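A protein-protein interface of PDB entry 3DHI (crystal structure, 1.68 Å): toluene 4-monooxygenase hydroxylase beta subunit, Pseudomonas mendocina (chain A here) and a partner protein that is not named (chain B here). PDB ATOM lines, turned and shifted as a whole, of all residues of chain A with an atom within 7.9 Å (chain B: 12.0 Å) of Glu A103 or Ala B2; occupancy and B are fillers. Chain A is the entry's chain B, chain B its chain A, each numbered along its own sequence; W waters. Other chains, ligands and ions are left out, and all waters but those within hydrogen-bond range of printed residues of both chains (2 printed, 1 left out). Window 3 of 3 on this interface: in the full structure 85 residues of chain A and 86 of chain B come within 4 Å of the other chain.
The backbone NH (N) of Ala B2 lies within hydrogen-bond range of the side-chain carboxylate (OD1) of Asp A99, at 2.7 Å. ND2 of Asn A102 lies close to N of Ala B2. The backbone NH of Ala B2 is in hydrogen-bond range of the side-chain carboxylate of Glu A103 (2.5 Å). The backbone NH (N) of Asp A99 lies within hydrogen-bond range of the side-chain sulfur (SD) of Met B3 (3.6 Å). The side-chain hydroxyl of Tyr A168 lies close to the side-chain sulfur of Met B3, at 3.7 Å. The side-chain hydroxyl (OH) of Tyr A168 sits at hydrogen-bond distance from the backbone NH (N) of His B4, at 3.0 Å. A ring nitrogen (ND1) of His B4 sits close to the side-chain carboxylate of Glu A172 (3.5 Å). The backbone carbonyl oxygen (O) of Gln A95 lies close to the side-chain sulfur (SD) of Met B3, 3.5 Å away.
O of His B4 lies within hydrogen-bond range of NE1 of Trp B9, 3.0 Å away. O of Pro B5 lies within hydrogen-bond range of NE1 of Trp B9, 3.2 Å away. The side-chain carboxylate of Glu A172 lies close to the side-chain amide oxygen of Asn A102, at 3.0 Å.
His B4 touches Asn A102 (CE1 to OD1, 3.5 Å). NE1 of Trp B9 touches CD1 of Tyr A168 (3.4 Å).
Printed residues of chain B within 4 Å of Glu A103: Ala B2 (2.5 Å). Ala B2 touches just these residues of chain A: Asp A99, Asn A102 and Glu A103. No residue of chain B comes within 4 Å of Arg A104. Glu A105 touches none of the printed residues of chain B. Of the printed residues of chain B, Gln A95 touches Met B3. Printed residues of chain A within 4 Å of Trp B9: Tyr A168. Printed residues of chain A within 4 Å of Met B3: Gln A95, Asp A99 and Tyr A168. Of the printed residues of chain B, Glu A172 touches His B4. Printed residues of chain B within 4 Å of Tyr A168: Met B3 (3.3 Å), His B4 (3.0 Å) and Trp B9 (3.4 Å). Phe A101 touches none of the printed residues of chain B. His A106 touches none of the printed residues of chain B. The nearest residue of chain B that does not touch Glu A103 is Met B3 (5.8 Å). The nearest printed residue of chain A that does not touch Ala B2 is Phe A98 (4.2 Å).
Of the 14 printed residues of chain A, 6 touch a printed residue of chain B. Printed residues of chain A that touch a printed residue of chain B: Gln A95, Asp A99, Asn A102, Glu A103, Tyr A168 and Glu A172. Hydrophobic or aromatic side chains of chain A that line the printed part of chain B: Tyr A168. Of the 7 printed residues of chain B, 4 touch a printed residue of chain A. Printed residues of chain B that touch a printed residue of chain A: Ala B2, Met B3, His B4 and Trp B9. Among the printed residues, 10 pairs touch across the chains. Among the printed residues, no Asp or Glu carboxylate lies within 4 Å of a Lys or Arg side-chain nitrogen of the other chain.
Water W2 bridges OD1 of Asn A102 and NE2 of His B4. Water W1 lies within hydrogen-bond range of the backbone carbonyl oxygen (O) of Gln A95 and the side-chain sulfur (SD) of Met B3.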
ATOM      1  N   GLN A  95      -2.613   3.661  13.418  1.00  0.00           N
ATOM      2  CA  GLN A  95      -2.956   4.746  12.485  1.00  0.00           C
ATOM      3  C   GLN A  95      -2.008   5.935  12.655  1.00  0.00           C
ATOM      4  O   GLN A  95      -1.673   6.605  11.681  1.00  0.00           O
ATOM      5  CB  GLN A  95      -4.413   5.182  12.664  1.00  0.00           C
ATOM      6  CG  GLN A  95      -5.440   4.063  12.375  1.00  0.00           C
ATOM      7  CD  GLN A  95      -5.491   3.622  10.905  1.00  0.00           C
ATOM      8  OE1 GLN A  95      -5.729   4.437  10.015  1.00  0.00           O
ATOM      9  NE2 GLN A  95      -5.326   2.310  10.659  1.00  0.00           N
ATOM     10  N   SER A  96      -1.580   6.204  13.892  1.00  0.00           N
ATOM     11  CA  SER A  96      -0.583   7.239  14.156  1.00  0.00           C
ATOM     12  C   SER A  96       0.779   6.881  13.572  1.00  0.00           C
ATOM     13  O   SER A  96       1.472   7.750  13.070  1.00  0.00           O
ATOM     14  CB  SER A  96      -0.463   7.564  15.652  1.00  0.00           C
ATOM     15  OG  SER A  96      -1.675   8.195  16.114  1.00  0.00           O
ATOM     16  N   LEU A  97       1.167   5.616  13.666  1.00  0.00           N
ATOM     17  CA  LEU A  97       2.387   5.159  12.984  1.00  0.00           C
ATOM     18  C   LEU A  97       2.281   5.411  11.476  1.00  0.00           C
ATOM     19  O   LEU A  97       3.230   5.926  10.860  1.00  0.00           O
ATOM     20  CB  LEU A  97       2.626   3.668  13.245  1.00  0.00           C
ATOM     21  CG  LEU A  97       3.115   3.312  14.648  1.00  0.00           C
ATOM     22  CD1 LEU A  97       3.118   1.783  14.741  1.00  0.00           C
ATOM     23  CD2 LEU A  97       4.475   3.897  15.015  1.00  0.00           C
ATOM     24  N   PHE A  98       1.146   5.018  10.880  1.00  0.00           N
ATOM     25  CA  PHE A  98       0.951   5.197   9.425  1.00  0.00           C
ATOM     26  C   PHE A  98       1.157   6.674   9.069  1.00  0.00           C
ATOM     27  O   PHE A  98       1.923   7.022   8.157  1.00  0.00           O
ATOM     28  CB  PHE A  98      -0.448   4.738   8.963  1.00  0.00           C
ATOM     29  CG  PHE A  98      -0.653   3.231   8.971  1.00  0.00           C
ATOM     30  CD1 PHE A  98      -1.934   2.717   8.810  1.00  0.00           C
ATOM     31  CD2 PHE A  98       0.408   2.338   9.140  1.00  0.00           C
ATOM     32  CE1 PHE A  98      -2.164   1.337   8.786  1.00  0.00           C
ATOM     33  CE2 PHE A  98       0.186   0.947   9.150  1.00  0.00           C
ATOM     34  CZ  PHE A  98      -1.111   0.448   8.967  1.00  0.00           C
ATOM     35  N   ASP A  99       0.500   7.543   9.823  1.00  0.00           N
ATOM     36  CA  ASP A  99       0.571   8.987   9.584  1.00  0.00           C
ATOM     37  C   ASP A  99       2.011   9.477   9.633  1.00  0.00           C
ATOM     38  O   ASP A  99       2.485  10.108   8.703  1.00  0.00           O
ATOM     39  CB  ASP A  99      -0.287   9.727  10.617  1.00  0.00           C
ATOM     40  CG  ASP A  99      -0.506  11.192  10.275  1.00  0.00           C
ATOM     41  OD1 ASP A  99      -0.244  11.609   9.129  1.00  0.00           O
ATOM     42  OD2 ASP A  99      -0.977  11.933  11.174  1.00  0.00           O
ATOM     43  N   GLN A 100       2.700   9.159  10.729  1.00  0.00           N
ATOM     44  CA  GLN A 100       4.057   9.614  11.003  1.00  0.00           C
ATOM     45  C   GLN A 100       5.057   9.074   9.975  1.00  0.00           C
ATOM     46  O   GLN A 100       5.918   9.815   9.478  1.00  0.00           O
ATOM     47  CB  GLN A 100       4.401   9.164  12.434  1.00  0.00           C
ATOM     48  CG  GLN A 100       5.863   9.053  12.814  1.00  0.00           C
ATOM     49  CD  GLN A 100       6.583  10.379  12.797  1.00  0.00           C
ATOM     50  OE1 GLN A 100       5.967  11.457  12.774  1.00  0.00           O
ATOM     51  NE2 GLN A 100       7.912  10.308  12.789  1.00  0.00           N
ATOM     52  N   PHE A 101       4.964   7.776   9.684  1.00  0.00           N
ATOM     53  CA  PHE A 101       5.916   7.160   8.746  1.00  0.00           C
ATOM     54  C   PHE A 101       5.682   7.692   7.334  1.00  0.00           C
ATOM     55  O   PHE A 101       6.620   7.885   6.556  1.00  0.00           O
ATOM     56  CB  PHE A 101       5.849   5.636   8.844  1.00  0.00           C
ATOM     57  CG  PHE A 101       6.639   5.079  10.006  1.00  0.00           C
ATOM     58  CD1 PHE A 101       7.821   4.367   9.778  1.00  0.00           C
ATOM     59  CD2 PHE A 101       6.250   5.310  11.331  1.00  0.00           C
ATOM     60  CE1 PHE A 101       8.573   3.838  10.858  1.00  0.00           C
ATOM     61  CE2 PHE A 101       7.000   4.795  12.415  1.00  0.00           C
ATOM     62  CZ  PHE A 101       8.176   4.060  12.165  1.00  0.00           C
ATOM     63  N   ASN A 102       4.423   7.964   7.004  1.00  0.00           N
ATOM     64  CA  ASN A 102       4.119   8.604   5.734  1.00  0.00           C
ATOM     65  C   ASN A 102       4.716  10.030   5.683  1.00  0.00           C
ATOM     66  O   ASN A 102       5.267  10.439   4.648  1.00  0.00           O
ATOM     67  CB  ASN A 102       2.602   8.619   5.489  1.00  0.00           C
ATOM     68  CG  ASN A 102       2.211   9.460   4.283  1.00  0.00           C
ATOM     69  OD1 ASN A 102       1.979   8.941   3.183  1.00  0.00           O
ATOM     70  ND2 ASN A 102       2.165  10.757   4.473  1.00  0.00           N
ATOM     71  N   GLU A 103       4.604  10.774   6.792  1.00  0.00           N
ATOM     72  CA  GLU A 103       5.184  12.141   6.882  1.00  0.00           C
ATOM     73  C   GLU A 103       6.683  12.105   6.611  1.00  0.00           C
ATOM     74  O   GLU A 103       7.225  12.987   5.927  1.00  0.00           O
ATOM     75  CB  GLU A 103       4.909  12.799   8.246  1.00  0.00           C
ATOM     76  CG  GLU A 103       3.461  13.274   8.446  1.00  0.00           C
ATOM     77  CD  GLU A 103       3.053  14.342   7.435  1.00  0.00           C
ATOM     78  OE1 GLU A 103       2.067  14.124   6.701  1.00  0.00           O
ATOM     79  OE2 GLU A 103       3.746  15.390   7.360  1.00  0.00           O
ATOM     80  N   ARG A 104       7.340  11.071   7.125  1.00  0.00           N
ATOM     81  CA  ARG A 104       8.789  10.927   6.998  1.00  0.00           C
ATOM     82  C   ARG A 104       9.209  10.253   5.693  1.00  0.00           C
ATOM     83  O   ARG A 104      10.407  10.022   5.469  1.00  0.00           O
ATOM     84  CB  ARG A 104       9.365  10.187   8.218  1.00  0.00           C
ATOM     85  CG  ARG A 104       9.377  11.034   9.494  1.00  0.00           C
ATOM     86  CD  ARG A 104      10.020  12.399   9.269  1.00  0.00           C
ATOM     87  NE  ARG A 104      10.228  13.150  10.508  1.00  0.00           N
ATOM     88  CZ  ARG A 104      10.865  14.317  10.583  1.00  0.00           C
ATOM     89  NH1 ARG A 104      11.368  14.884   9.490  1.00  0.00           N
ATOM     90  NH2 ARG A 104      11.007  14.921  11.757  1.00  0.00           N
ATOM     91  N   GLU A 105       8.230   9.945   4.833  1.00  0.00           N
ATOM     92  CA  GLU A 105       8.480   9.283   3.541  1.00  0.00           C
ATOM     93  C   GLU A 105       9.260   7.965   3.709  1.00  0.00           C
ATOM     94  O   GLU A 105      10.215   7.670   2.973  1.00  0.00           O
ATOM     95  CB  GLU A 105       9.159  10.248   2.559  1.00  0.00           C
ATOM     96  CG  GLU A 105       8.321  11.481   2.236  1.00  0.00           C
ATOM     97  CD  GLU A 105       9.108  12.544   1.479  1.00  0.00           C
ATOM     98  OE1 GLU A 105      10.359  12.589   1.608  1.00  0.00           O
ATOM     99  OE2 GLU A 105       8.465  13.343   0.757  1.00  0.00           O
ATOM    100  N   HIS A 106       8.831   7.174   4.691  1.00  0.00           N
ATOM    101  CA  HIS A 106       9.423   5.875   4.982  1.00  0.00           C
ATOM    102  C   HIS A 106       9.540   4.986   3.742  1.00  0.00           C
ATOM    103  O   HIS A 106      10.567   4.338   3.519  1.00  0.00           O
ATOM    104  CB  HIS A 106       8.595   5.158   6.063  1.00  0.00           C
ATOM    105  CG  HIS A 106       8.894   3.692   6.197  1.00  0.00           C
ATOM    106  ND1 HIS A 106       8.327   2.739   5.380  1.00  0.00           N
ATOM    107  CD2 HIS A 106       9.697   3.020   7.058  1.00  0.00           C
ATOM    108  CE1 HIS A 106       8.753   1.541   5.743  1.00  0.00           C
ATOM    109  NE2 HIS A 106       9.584   1.686   6.759  1.00  0.00           N
ATOM    110  N   TYR A 168      -4.804  -1.100   3.370  1.00  0.00           N
ATOM    111  CA  TYR A 168      -4.374   0.283   3.470  1.00  0.00           C
ATOM    112  C   TYR A 168      -2.910   0.382   3.033  1.00  0.00           C
ATOM    113  O   TYR A 168      -2.536   1.291   2.296  1.00  0.00           O
ATOM    114  CB  TYR A 168      -4.509   0.760   4.903  1.00  0.00           C
ATOM    115  CG  TYR A 168      -4.129   2.220   5.049  1.00  0.00           C
ATOM    116  CD1 TYR A 168      -5.108   3.224   4.936  1.00  0.00           C
ATOM    117  CD2 TYR A 168      -2.810   2.600   5.310  1.00  0.00           C
ATOM    118  CE1 TYR A 168      -4.774   4.570   5.069  1.00  0.00           C
ATOM    119  CE2 TYR A 168      -2.459   3.951   5.436  1.00  0.00           C
ATOM    120  CZ  TYR A 168      -3.450   4.932   5.317  1.00  0.00           C
ATOM    121  OH  TYR A 168      -3.109   6.262   5.453  1.00  0.00           O
ATOM    122  N   GLU A 172      -1.095   2.327  -0.032  1.00  0.00           N
ATOM    123  CA  GLU A 172      -0.121   3.359   0.275  1.00  0.00           C
ATOM    124  C   GLU A 172       1.201   3.082  -0.433  1.00  0.00           C
ATOM    125  O   GLU A 172       1.760   3.980  -1.050  1.00  0.00           O
ATOM    126  CB  GLU A 172       0.103   3.457   1.774  1.00  0.00           C
ATOM    127  CG  GLU A 172       1.092   4.565   2.117  1.00  0.00           C
ATOM    128  CD  GLU A 172       1.038   4.946   3.567  1.00  0.00           C
ATOM    129  OE1 GLU A 172       0.963   6.168   3.828  1.00  0.00           O
ATOM    130  OE2 GLU A 172       1.071   4.041   4.428  1.00  0.00           O
ATOM    131  N   ALA B   2       0.785  11.973   6.624  1.00  0.00           N
ATOM    132  CA  ALA B   2      -0.596  12.064   6.071  1.00  0.00           C
ATOM    133  C   ALA B   2      -1.294  10.713   6.037  1.00  0.00           C
ATOM    134  O   ALA B   2      -0.644   9.666   6.057  1.00  0.00           O
ATOM    135  CB  ALA B   2      -0.588  12.696   4.666  1.00  0.00           C
ATOM    136  N   MET B   3      -2.625  10.767   6.009  1.00  0.00           N
ATOM    137  CA  MET B   3      -3.484   9.594   5.888  1.00  0.00           C
ATOM    138  C   MET B   3      -4.234   9.650   4.565  1.00  0.00           C
ATOM    139  O   MET B   3      -4.632  10.746   4.086  1.00  0.00           O
ATOM    140  CB  MET B   3      -4.514   9.540   7.029  1.00  0.00           C
ATOM    141  CG  MET B   3      -3.919   9.501   8.439  1.00  0.00           C
ATOM    142  SD  MET B   3      -2.858   8.059   8.693  1.00  0.00           S
ATOM    143  CE  MET B   3      -4.024   6.713   8.640  1.00  0.00           C
ATOM    144  N   HIS B   4      -4.492   8.476   4.004  1.00  0.00           N
ATOM    145  CA  HIS B   4      -5.224   8.397   2.749  1.00  0.00           C
ATOM    146  C   HIS B   4      -6.691   8.112   3.003  1.00  0.00           C
ATOM    147  O   HIS B   4      -7.013   7.316   3.878  1.00  0.00           O
ATOM    148  CB  HIS B   4      -4.559   7.373   1.860  1.00  0.00           C
ATOM    149  CG  HIS B   4      -3.093   7.635   1.736  1.00  0.00           C
ATOM    150  ND1 HIS B   4      -2.130   6.859   2.345  1.00  0.00           N
ATOM    151  CD2 HIS B   4      -2.443   8.690   1.193  1.00  0.00           C
ATOM    152  CE1 HIS B   4      -0.940   7.391   2.120  1.00  0.00           C
ATOM    153  NE2 HIS B   4      -1.103   8.503   1.425  1.00  0.00           N
ATOM    154  N   PRO B   5      -7.578   8.787   2.243  1.00  0.00           N
ATOM    155  CA  PRO B   5      -9.011   8.669   2.532  1.00  0.00           C
ATOM    156  C   PRO B   5      -9.556   7.292   2.189  1.00  0.00           C
ATOM    157  O   PRO B   5      -9.056   6.601   1.283  1.00  0.00           O
ATOM    158  CB  PRO B   5      -9.652   9.732   1.631  1.00  0.00           C
ATOM    159  CG  PRO B   5      -8.707   9.871   0.492  1.00  0.00           C
ATOM    160  CD  PRO B   5      -7.319   9.656   1.076  1.00  0.00           C
ATOM    161  N   ARG B   6     -10.619   6.923   2.886  1.00  0.00           N
ATOM    162  CA  ARG B   6     -11.185   5.589   2.735  1.00  0.00           C
ATOM    163  C   ARG B   6     -11.516   5.250   1.290  1.00  0.00           C
ATOM    164  O   ARG B   6     -11.313   4.111   0.873  1.00  0.00           O
ATOM    165  CB  ARG B   6     -12.449   5.443   3.600  1.00  0.00           C
ATOM    166  CG  ARG B   6     -12.912   4.016   3.740  1.00  0.00           C
ATOM    167  CD  ARG B   6     -14.187   3.924   4.619  1.00  0.00           C
ATOM    168  NE  ARG B   6     -15.333   4.523   3.949  1.00  0.00           N
ATOM    169  CZ  ARG B   6     -16.454   4.898   4.576  1.00  0.00           C
ATOM    170  NH1 ARG B   6     -16.574   4.722   5.884  1.00  0.00           N
ATOM    171  NH2 ARG B   6     -17.463   5.444   3.885  1.00  0.00           N
ATOM    172  N   ASP B   8     -10.050   5.725  -1.326  1.00  0.00           N
ATOM    173  CA  ASP B   8      -8.879   5.312  -2.114  1.00  0.00           C
ATOM    174  C   ASP B   8      -8.414   3.883  -1.862  1.00  0.00           C
ATOM    175  O   ASP B   8      -7.777   3.288  -2.741  1.00  0.00           O
ATOM    176  CB  ASP B   8      -7.715   6.273  -1.923  1.00  0.00           C
ATOM    177  CG  ASP B   8      -8.005   7.671  -2.470  1.00  0.00           C
ATOM    178  OD1 ASP B   8      -9.034   7.862  -3.151  1.00  0.00           O
ATOM    179  OD2 ASP B   8      -7.190   8.575  -2.218  1.00  0.00           O
ATOM    180  N   TRP B   9      -8.718   3.330  -0.686  1.00  0.00           N
ATOM    181  CA  TRP B   9      -8.301   1.949  -0.360  1.00  0.00           C
ATOM    182  C   TRP B   9      -9.454   1.001  -0.029  1.00  0.00           C
ATOM    183  O   TRP B   9      -9.233  -0.208   0.203  1.00  0.00           O
ATOM    184  CB  TRP B   9      -7.267   1.933   0.784  1.00  0.00           C
ATOM    185  CG  TRP B   9      -7.651   2.761   1.971  1.00  0.00           C
ATOM    186  CD1 TRP B   9      -7.281   4.045   2.207  1.00  0.00           C
ATOM    187  CD2 TRP B   9      -8.498   2.369   3.072  1.00  0.00           C
ATOM    188  NE1 TRP B   9      -7.851   4.497   3.379  1.00  0.00           N
ATOM    189  CE2 TRP B   9      -8.605   3.488   3.929  1.00  0.00           C
ATOM    190  CE3 TRP B   9      -9.187   1.188   3.402  1.00  0.00           C
ATOM    191  CZ2 TRP B   9      -9.372   3.469   5.111  1.00  0.00           C
ATOM    192  CZ3 TRP B   9      -9.984   1.171   4.569  1.00  0.00           C
ATOM    193  CH2 TRP B   9     -10.050   2.307   5.417  1.00  0.00           C
HETATM  194  O   HOH W   1      -3.909   8.719  11.900  1.00  0.00           O
HETATM  195  O   HOH W   2       1.374  10.661   0.741  1.00  0.00           O
